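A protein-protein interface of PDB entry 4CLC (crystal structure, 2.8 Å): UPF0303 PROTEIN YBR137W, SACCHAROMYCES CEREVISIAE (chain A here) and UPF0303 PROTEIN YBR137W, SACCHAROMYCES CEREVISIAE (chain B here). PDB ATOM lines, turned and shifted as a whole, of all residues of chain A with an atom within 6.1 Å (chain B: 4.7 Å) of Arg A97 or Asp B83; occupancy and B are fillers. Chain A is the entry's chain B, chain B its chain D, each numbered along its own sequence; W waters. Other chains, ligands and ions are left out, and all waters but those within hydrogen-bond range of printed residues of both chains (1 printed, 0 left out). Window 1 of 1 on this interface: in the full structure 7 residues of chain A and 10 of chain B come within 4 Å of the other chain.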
ATOM      1  N   LYS A  92      -9.097 -13.766 -24.004  1.00  0.00           N
ATOM      2  CA  LYS A  92     -10.060 -12.755 -24.450  1.00  0.00           C
ATOM      3  C   LYS A  92      -9.426 -11.374 -24.430  1.00  0.00           C
ATOM      4  O   LYS A  92      -9.549 -10.616 -25.384  1.00  0.00           O
ATOM      5  CB  LYS A  92     -11.322 -12.766 -23.580  1.00  0.00           C
ATOM      6  CG  LYS A  92     -12.403 -11.751 -23.994  1.00  0.00           C
ATOM      7  CD  LYS A  92     -13.537 -11.655 -22.959  1.00  0.00           C
ATOM      8  CE  LYS A  92     -13.003 -11.340 -21.557  1.00  0.00           C
ATOM      9  NZ  LYS A  92     -14.075 -11.306 -20.515  1.00  0.00           N
ATOM     10  N   LYS A  93      -8.722 -11.070 -23.348  1.00  0.00           N
ATOM     11  CA  LYS A  93      -8.118  -9.759 -23.178  1.00  0.00           C
ATOM     12  C   LYS A  93      -7.122  -9.471 -24.287  1.00  0.00           C
ATOM     13  O   LYS A  93      -7.058  -8.361 -24.808  1.00  0.00           O
ATOM     14  CB  LYS A  93      -7.447  -9.672 -21.809  1.00  0.00           C
ATOM     15  CG  LYS A  93      -7.230  -8.248 -21.304  1.00  0.00           C
ATOM     16  CD  LYS A  93      -6.915  -8.249 -19.819  1.00  0.00           C
ATOM     17  CE  LYS A  93      -6.831  -6.848 -19.270  1.00  0.00           C
ATOM     18  NZ  LYS A  93      -6.588  -6.908 -17.806  1.00  0.00           N
ATOM     19  N   THR A  94      -6.354 -10.493 -24.648  1.00  0.00           N
ATOM     20  CA  THR A  94      -5.427 -10.406 -25.769  1.00  0.00           C
ATOM     21  C   THR A  94      -6.158 -10.107 -27.068  1.00  0.00           C
ATOM     22  O   THR A  94      -5.844  -9.143 -27.778  1.00  0.00           O
ATOM     23  CB  THR A  94      -4.648 -11.709 -25.956  1.00  0.00           C
ATOM     24  OG1 THR A  94      -3.844 -11.958 -24.799  1.00  0.00           O
ATOM     25  CG2 THR A  94      -3.753 -11.598 -27.164  1.00  0.00           C
ATOM     26  N   ALA A  95      -7.136 -10.951 -27.375  1.00  0.00           N
ATOM     27  CA  ALA A  95      -7.897 -10.800 -28.598  1.00  0.00           C
ATOM     28  C   ALA A  95      -8.586  -9.436 -28.644  1.00  0.00           C
ATOM     29  O   ALA A  95      -8.583  -8.772 -29.675  1.00  0.00           O
ATOM     30  CB  ALA A  95      -8.907 -11.923 -28.731  1.00  0.00           C
ATOM     31  N   LEU A  96      -9.146  -9.009 -27.514  1.00  0.00           N
ATOM     32  CA  LEU A  96      -9.824  -7.708 -27.446  1.00  0.00           C
ATOM     33  C   LEU A  96      -8.860  -6.544 -27.535  1.00  0.00           C
ATOM     34  O   LEU A  96      -9.182  -5.522 -28.150  1.00  0.00           O
ATOM     35  CB  LEU A  96     -10.643  -7.588 -26.173  1.00  0.00           C
ATOM     36  CG  LEU A  96     -12.012  -8.173 -26.450  1.00  0.00           C
ATOM     37  CD1 LEU A  96     -12.800  -8.285 -25.187  1.00  0.00           C
ATOM     38  CD2 LEU A  96     -12.698  -7.276 -27.452  1.00  0.00           C
ATOM     39  N   ARG A  97      -7.677  -6.700 -26.942  1.00  0.00           N
ATOM     40  CA  ARG A  97      -6.710  -5.611 -26.910  1.00  0.00           C
ATOM     41  C   ARG A  97      -5.973  -5.412 -28.232  1.00  0.00           C
ATOM     42  O   ARG A  97      -5.838  -4.289 -28.687  1.00  0.00           O
ATOM     43  CB  ARG A  97      -5.692  -5.819 -25.798  1.00  0.00           C
ATOM     44  CG  ARG A  97      -4.615  -4.779 -25.868  1.00  0.00           C
ATOM     45  CD  ARG A  97      -3.647  -4.862 -24.738  1.00  0.00           C
ATOM     46  NE  ARG A  97      -2.483  -4.073 -25.090  1.00  0.00           N
ATOM     47  CZ  ARG A  97      -1.562  -3.666 -24.234  1.00  0.00           C
ATOM     48  NH1 ARG A  97      -1.676  -3.955 -22.944  1.00  0.00           N
ATOM     49  NH2 ARG A  97      -0.541  -2.946 -24.681  1.00  0.00           N
ATOM     50  N   PHE A  98      -5.481  -6.479 -28.852  1.00  0.00           N
ATOM     51  CA  PHE A  98      -4.800  -6.314 -30.145  1.00  0.00           C
ATOM     52  C   PHE A  98      -5.844  -6.480 -31.233  1.00  0.00           C
ATOM     53  O   PHE A  98      -7.006  -6.809 -30.953  1.00  0.00           O
ATOM     54  CB  PHE A  98      -3.637  -7.310 -30.289  1.00  0.00           C
ATOM     55  CG  PHE A  98      -2.625  -7.221 -29.156  1.00  0.00           C
ATOM     56  CD1 PHE A  98      -2.813  -7.932 -27.977  1.00  0.00           C
ATOM     57  CD2 PHE A  98      -1.515  -6.377 -29.259  1.00  0.00           C
ATOM     58  CE1 PHE A  98      -1.916  -7.809 -26.934  1.00  0.00           C
ATOM     59  CE2 PHE A  98      -0.605  -6.256 -28.218  1.00  0.00           C
ATOM     60  CZ  PHE A  98      -0.807  -6.971 -27.056  1.00  0.00           C
ATOM     61  N   GLY A  99      -5.475  -6.271 -32.479  1.00  0.00           N
ATOM     62  CA  GLY A  99      -6.523  -6.314 -33.486  1.00  0.00           C
ATOM     63  C   GLY A  99      -7.002  -7.705 -33.883  1.00  0.00           C
ATOM     64  O   GLY A  99      -7.802  -7.854 -34.800  1.00  0.00           O
ATOM     65  N   HIS A 100      -6.506  -8.730 -33.200  1.00  0.00           N
ATOM     66  CA  HIS A 100      -6.445 -10.051 -33.801  1.00  0.00           C
ATOM     67  C   HIS A 100      -6.823 -11.130 -32.817  1.00  0.00           C
ATOM     68  O   HIS A 100      -7.065 -10.853 -31.656  1.00  0.00           O
ATOM     69  CB  HIS A 100      -5.035 -10.325 -34.347  1.00  0.00           C
ATOM     70  CG  HIS A 100      -4.551  -9.308 -35.337  1.00  0.00           C
ATOM     71  ND1 HIS A 100      -5.061  -9.208 -36.616  1.00  0.00           N
ATOM     72  CD2 HIS A 100      -3.606  -8.344 -35.235  1.00  0.00           C
ATOM     73  CE1 HIS A 100      -4.450  -8.229 -37.261  1.00  0.00           C
ATOM     74  NE2 HIS A 100      -3.566  -7.682 -36.442  1.00  0.00           N
ATOM     75  N   PHE A 118       5.651  -7.788 -26.545  1.00  0.00           N
ATOM     76  CA  PHE A 118       4.558  -6.835 -26.426  1.00  0.00           C
ATOM     77  C   PHE A 118       4.486  -6.006 -25.161  1.00  0.00           C
ATOM     78  O   PHE A 118       3.623  -5.156 -25.057  1.00  0.00           O
ATOM     79  CB  PHE A 118       3.260  -7.589 -26.591  1.00  0.00           C
ATOM     80  CG  PHE A 118       3.215  -8.361 -27.848  1.00  0.00           C
ATOM     81  CD1 PHE A 118       3.287  -7.701 -29.067  1.00  0.00           C
ATOM     82  CD2 PHE A 118       3.132  -9.738 -27.828  1.00  0.00           C
ATOM     83  CE1 PHE A 118       3.260  -8.404 -30.249  1.00  0.00           C
ATOM     84  CE2 PHE A 118       3.095 -10.453 -29.002  1.00  0.00           C
ATOM     85  CZ  PHE A 118       3.156  -9.787 -30.218  1.00  0.00           C
ATOM     86  N   PHE A 119       5.369  -6.277 -24.208  1.00  0.00           N
ATOM     87  CA  PHE A 119       5.453  -5.525 -22.953  1.00  0.00           C
ATOM     88  C   PHE A 119       4.245  -5.620 -22.051  1.00  0.00           C
ATOM     89  O   PHE A 119       3.989  -4.716 -21.274  1.00  0.00           O
ATOM     90  CB  PHE A 119       5.723  -4.065 -23.247  1.00  0.00           C
ATOM     91  CG  PHE A 119       6.956  -3.843 -24.055  1.00  0.00           C
ATOM     92  CD1 PHE A 119       8.190  -3.720 -23.436  1.00  0.00           C
ATOM     93  CD2 PHE A 119       6.889  -3.766 -25.434  1.00  0.00           C
ATOM     94  CE1 PHE A 119       9.316  -3.506 -24.170  1.00  0.00           C
ATOM     95  CE2 PHE A 119       8.026  -3.555 -26.171  1.00  0.00           C
ATOM     96  CZ  PHE A 119       9.238  -3.424 -25.537  1.00  0.00           C
ATOM     97  N   VAL A 120       3.531  -6.732 -22.118  1.00  0.00           N
ATOM     98  CA  VAL A 120       2.346  -6.921 -21.299  1.00  0.00           C
ATOM     99  C   VAL A 120       2.639  -8.061 -20.346  1.00  0.00           C
ATOM    100  O   VAL A 120       3.556  -8.805 -20.581  1.00  0.00           O
ATOM    101  CB  VAL A 120       1.108  -7.208 -22.155  1.00  0.00           C
ATOM    102  CG1 VAL A 120       0.905  -6.078 -23.136  1.00  0.00           C
ATOM    103  CG2 VAL A 120       1.250  -8.532 -22.887  1.00  0.00           C
ATOM    104  N   TYR A 125      -2.417 -11.487 -19.824  1.00  0.00           N
ATOM    105  CA  TYR A 125      -2.716 -11.724 -21.238  1.00  0.00           C
ATOM    106  C   TYR A 125      -2.235 -13.080 -21.749  1.00  0.00           C
ATOM    107  O   TYR A 125      -1.051 -13.382 -21.634  1.00  0.00           O
ATOM    108  CB  TYR A 125      -2.060 -10.658 -22.088  1.00  0.00           C
ATOM    109  CG  TYR A 125      -2.602  -9.271 -21.926  1.00  0.00           C
ATOM    110  CD1 TYR A 125      -2.128  -8.421 -20.923  1.00  0.00           C
ATOM    111  CD2 TYR A 125      -3.550  -8.783 -22.806  1.00  0.00           C
ATOM    112  CE1 TYR A 125      -2.613  -7.142 -20.794  1.00  0.00           C
ATOM    113  CE2 TYR A 125      -4.033  -7.506 -22.687  1.00  0.00           C
ATOM    114  CZ  TYR A 125      -3.564  -6.690 -21.688  1.00  0.00           C
ATOM    115  OH  TYR A 125      -4.071  -5.418 -21.594  1.00  0.00           O
ATOM    116  N   ALA B  81      -6.258  -0.305 -32.853  1.00  0.00           N
ATOM    117  CA  ALA B  81      -6.673  -1.088 -31.693  1.00  0.00           C
ATOM    118  C   ALA B  81      -6.219  -0.443 -30.407  1.00  0.00           C
ATOM    119  O   ALA B  81      -5.352   0.417 -30.414  1.00  0.00           O
ATOM    120  CB  ALA B  81      -6.144  -2.506 -31.779  1.00  0.00           C
ATOM    121  N   LEU B  82      -6.779  -0.909 -29.301  1.00  0.00           N
ATOM    122  CA  LEU B  82      -6.181  -0.689 -28.000  1.00  0.00           C
ATOM    123  C   LEU B  82      -4.782  -1.293 -28.121  1.00  0.00           C
ATOM    124  O   LEU B  82      -4.531  -2.119 -29.004  1.00  0.00           O
ATOM    125  CB  LEU B  82      -7.006  -1.382 -26.912  1.00  0.00           C
ATOM    126  CG  LEU B  82      -6.864  -1.102 -25.415  1.00  0.00           C
ATOM    127  CD1 LEU B  82      -7.202   0.344 -25.061  1.00  0.00           C
ATOM    128  CD2 LEU B  82      -7.771  -2.056 -24.696  1.00  0.00           C
ATOM    129  N   ASP B  83      -3.872  -0.873 -27.262  1.00  0.00           N
ATOM    130  CA  ASP B  83      -2.426  -1.153 -27.400  1.00  0.00           C
ATOM    131  C   ASP B  83      -1.799  -0.155 -28.374  1.00  0.00           C
ATOM    132  O   ASP B  83      -0.650   0.243 -28.169  1.00  0.00           O
ATOM    133  CB  ASP B  83      -2.167  -2.621 -27.846  1.00  0.00           C
ATOM    134  CG  ASP B  83      -0.747  -2.873 -28.282  1.00  0.00           C
ATOM    135  OD1 ASP B  83       0.109  -3.153 -27.412  1.00  0.00           O
ATOM    136  OD2 ASP B  83      -0.493  -2.821 -29.507  1.00  0.00           O
ATOM    137  N   ASN B  84      -2.585   0.417 -29.282  1.00  0.00           N
ATOM    138  CA  ASN B  84      -2.131   1.658 -29.873  1.00  0.00           C
ATOM    139  C   ASN B  84      -2.128   2.717 -28.793  1.00  0.00           C
ATOM    140  O   ASN B  84      -1.279   3.596 -28.767  1.00  0.00           O
ATOM    141  CB  ASN B  84      -3.002   2.095 -31.036  1.00  0.00           C
ATOM    142  CG  ASN B  84      -2.679   1.362 -32.308  1.00  0.00           C
ATOM    143  OD1 ASN B  84      -3.519   0.646 -32.848  1.00  0.00           O
ATOM    144  ND2 ASN B  84      -1.457   1.537 -32.803  1.00  0.00           N
ATOM    145  N   ASP B  85      -3.086   2.607 -27.881  1.00  0.00           N
ATOM    146  CA  ASP B  85      -3.207   3.562 -26.786  1.00  0.00           C
ATOM    147  C   ASP B  85      -2.116   3.328 -25.747  1.00  0.00           C
ATOM    148  O   ASP B  85      -1.479   4.278 -25.274  1.00  0.00           O
ATOM    149  CB  ASP B  85      -4.594   3.478 -26.147  1.00  0.00           C
ATOM    150  CG  ASP B  85      -5.693   3.964 -27.068  1.00  0.00           C
ATOM    151  OD1 ASP B  85      -5.440   4.811 -27.957  1.00  0.00           O
ATOM    152  OD2 ASP B  85      -6.825   3.487 -26.921  1.00  0.00           O
ATOM    153  N   PHE B  86      -1.900   2.064 -25.401  1.00  0.00           N
ATOM    154  CA  PHE B  86      -0.803   1.706 -24.524  1.00  0.00           C
ATOM    155  C   PHE B  86       0.536   2.216 -25.081  1.00  0.00           C
ATOM    156  O   PHE B  86       1.311   2.850 -24.361  1.00  0.00           O
ATOM    157  CB  PHE B  86      -0.762   0.198 -24.329  1.00  0.00           C
ATOM    158  CG  PHE B  86      -1.828  -0.320 -23.424  1.00  0.00           C
ATOM    159  CD1 PHE B  86      -1.636  -0.333 -22.043  1.00  0.00           C
ATOM    160  CD2 PHE B  86      -3.032  -0.797 -23.941  1.00  0.00           C
ATOM    161  CE1 PHE B  86      -2.614  -0.802 -21.186  1.00  0.00           C
ATOM    162  CE2 PHE B  86      -4.023  -1.280 -23.091  1.00  0.00           C
ATOM    163  CZ  PHE B  86      -3.802  -1.277 -21.701  1.00  0.00           C
ATOM    164  N   TRP B  87       0.784   1.957 -26.368  1.00  0.00           N
ATOM    165  CA  TRP B  87       2.037   2.373 -26.991  1.00  0.00           C
ATOM    166  C   TRP B  87       2.152   3.875 -26.949  1.00  0.00           C
ATOM    167  O   TRP B  87       3.216   4.413 -26.624  1.00  0.00           O
ATOM    168  CB  TRP B  87       2.159   1.861 -28.440  1.00  0.00           C
ATOM    169  CG  TRP B  87       2.756   0.479 -28.496  1.00  0.00           C
ATOM    170  CD1 TRP B  87       2.085  -0.709 -28.612  1.00  0.00           C
ATOM    171  CD2 TRP B  87       4.132   0.146 -28.383  1.00  0.00           C
ATOM    172  NE1 TRP B  87       2.961  -1.758 -28.575  1.00  0.00           N
ATOM    173  CE2 TRP B  87       4.236  -1.257 -28.440  1.00  0.00           C
ATOM    174  CE3 TRP B  87       5.300   0.898 -28.242  1.00  0.00           C
ATOM    175  CZ2 TRP B  87       5.457  -1.923 -28.369  1.00  0.00           C
ATOM    176  CZ3 TRP B  87       6.512   0.238 -28.167  1.00  0.00           C
ATOM    177  CH2 TRP B  87       6.581  -1.157 -28.231  1.00  0.00           C
HETATM  178  O   HOH W   1      -8.817  -2.862 -29.155  1.00  0.00           O
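Arg A97 touches Ala B81. Arg A97 touches Phe B86. Phe A98 touches Asp B83 (CE2 to OD1, 3.3 Å). Gly A99 touches Ala B81 (N to CB, 3.9 Å). Phe A119 touches Trp B87 (CE2 to CH2, 3.5 Å).
Water W1 lies within hydrogen-bond range of the backbone NH (N) of Leu B82 (2.8 Å), the backbone carbonyl oxygen (O) of Leu A96 (2.9 Å) and the backbone carbonyl oxygen (O) of Arg A97 (3.3 Å).
Lys A92 touches none of the printed residues of chain B. Arg A97 touches four residues of chain B. Of the printed residues of chain B, Phe A119 touches Trp B87 (3.5 Å). Val A120 touches none of the printed residues of chain B. Of the printed residues of chain A, Leu B82 touches Arg A97 (2.6 Å). Asp B83 touches two residues of chain A. The nearest residue of chain A that does not touch Asp B83 is Phe A118 (4.7 Å). The nearest printed residue of chain A that does not touch Trp B87 is Phe A118 (4.9 Å).
The backbone carbonyl oxygen (O) of Arg A97 sits close to the backbone carbonyl oxygen (O) of Leu B82 (2.6 Å). NH2 of Arg A97 lies within salt-bridge range of OD1 of Asp B83, 2.8 Å away.
The side-chain hydroxyl of Tyr A125 is in hydrogen-bond range of the guanidinium group of Arg A97, at 3.1 Å. OD1 of Asn B84 is in hydrogen-bond range of N of Ala B81. The side-chain carboxylate (OD1) of Asp B83 sits close to the indole nitrogen (NE1) of Trp B87 (3.4 Å).
Hydrophobic or aromatic side chains of chain A within 4 Å of the printed part of chain B: Phe A98 and Phe A119. Among the printed residues, 7 pairs touch across the chains. Among the printed residues, Asp or Glu carboxylates within 4 Å of a Lys or Arg side-chain nitrogen of the other chain: Arg A97 with Asp B83.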
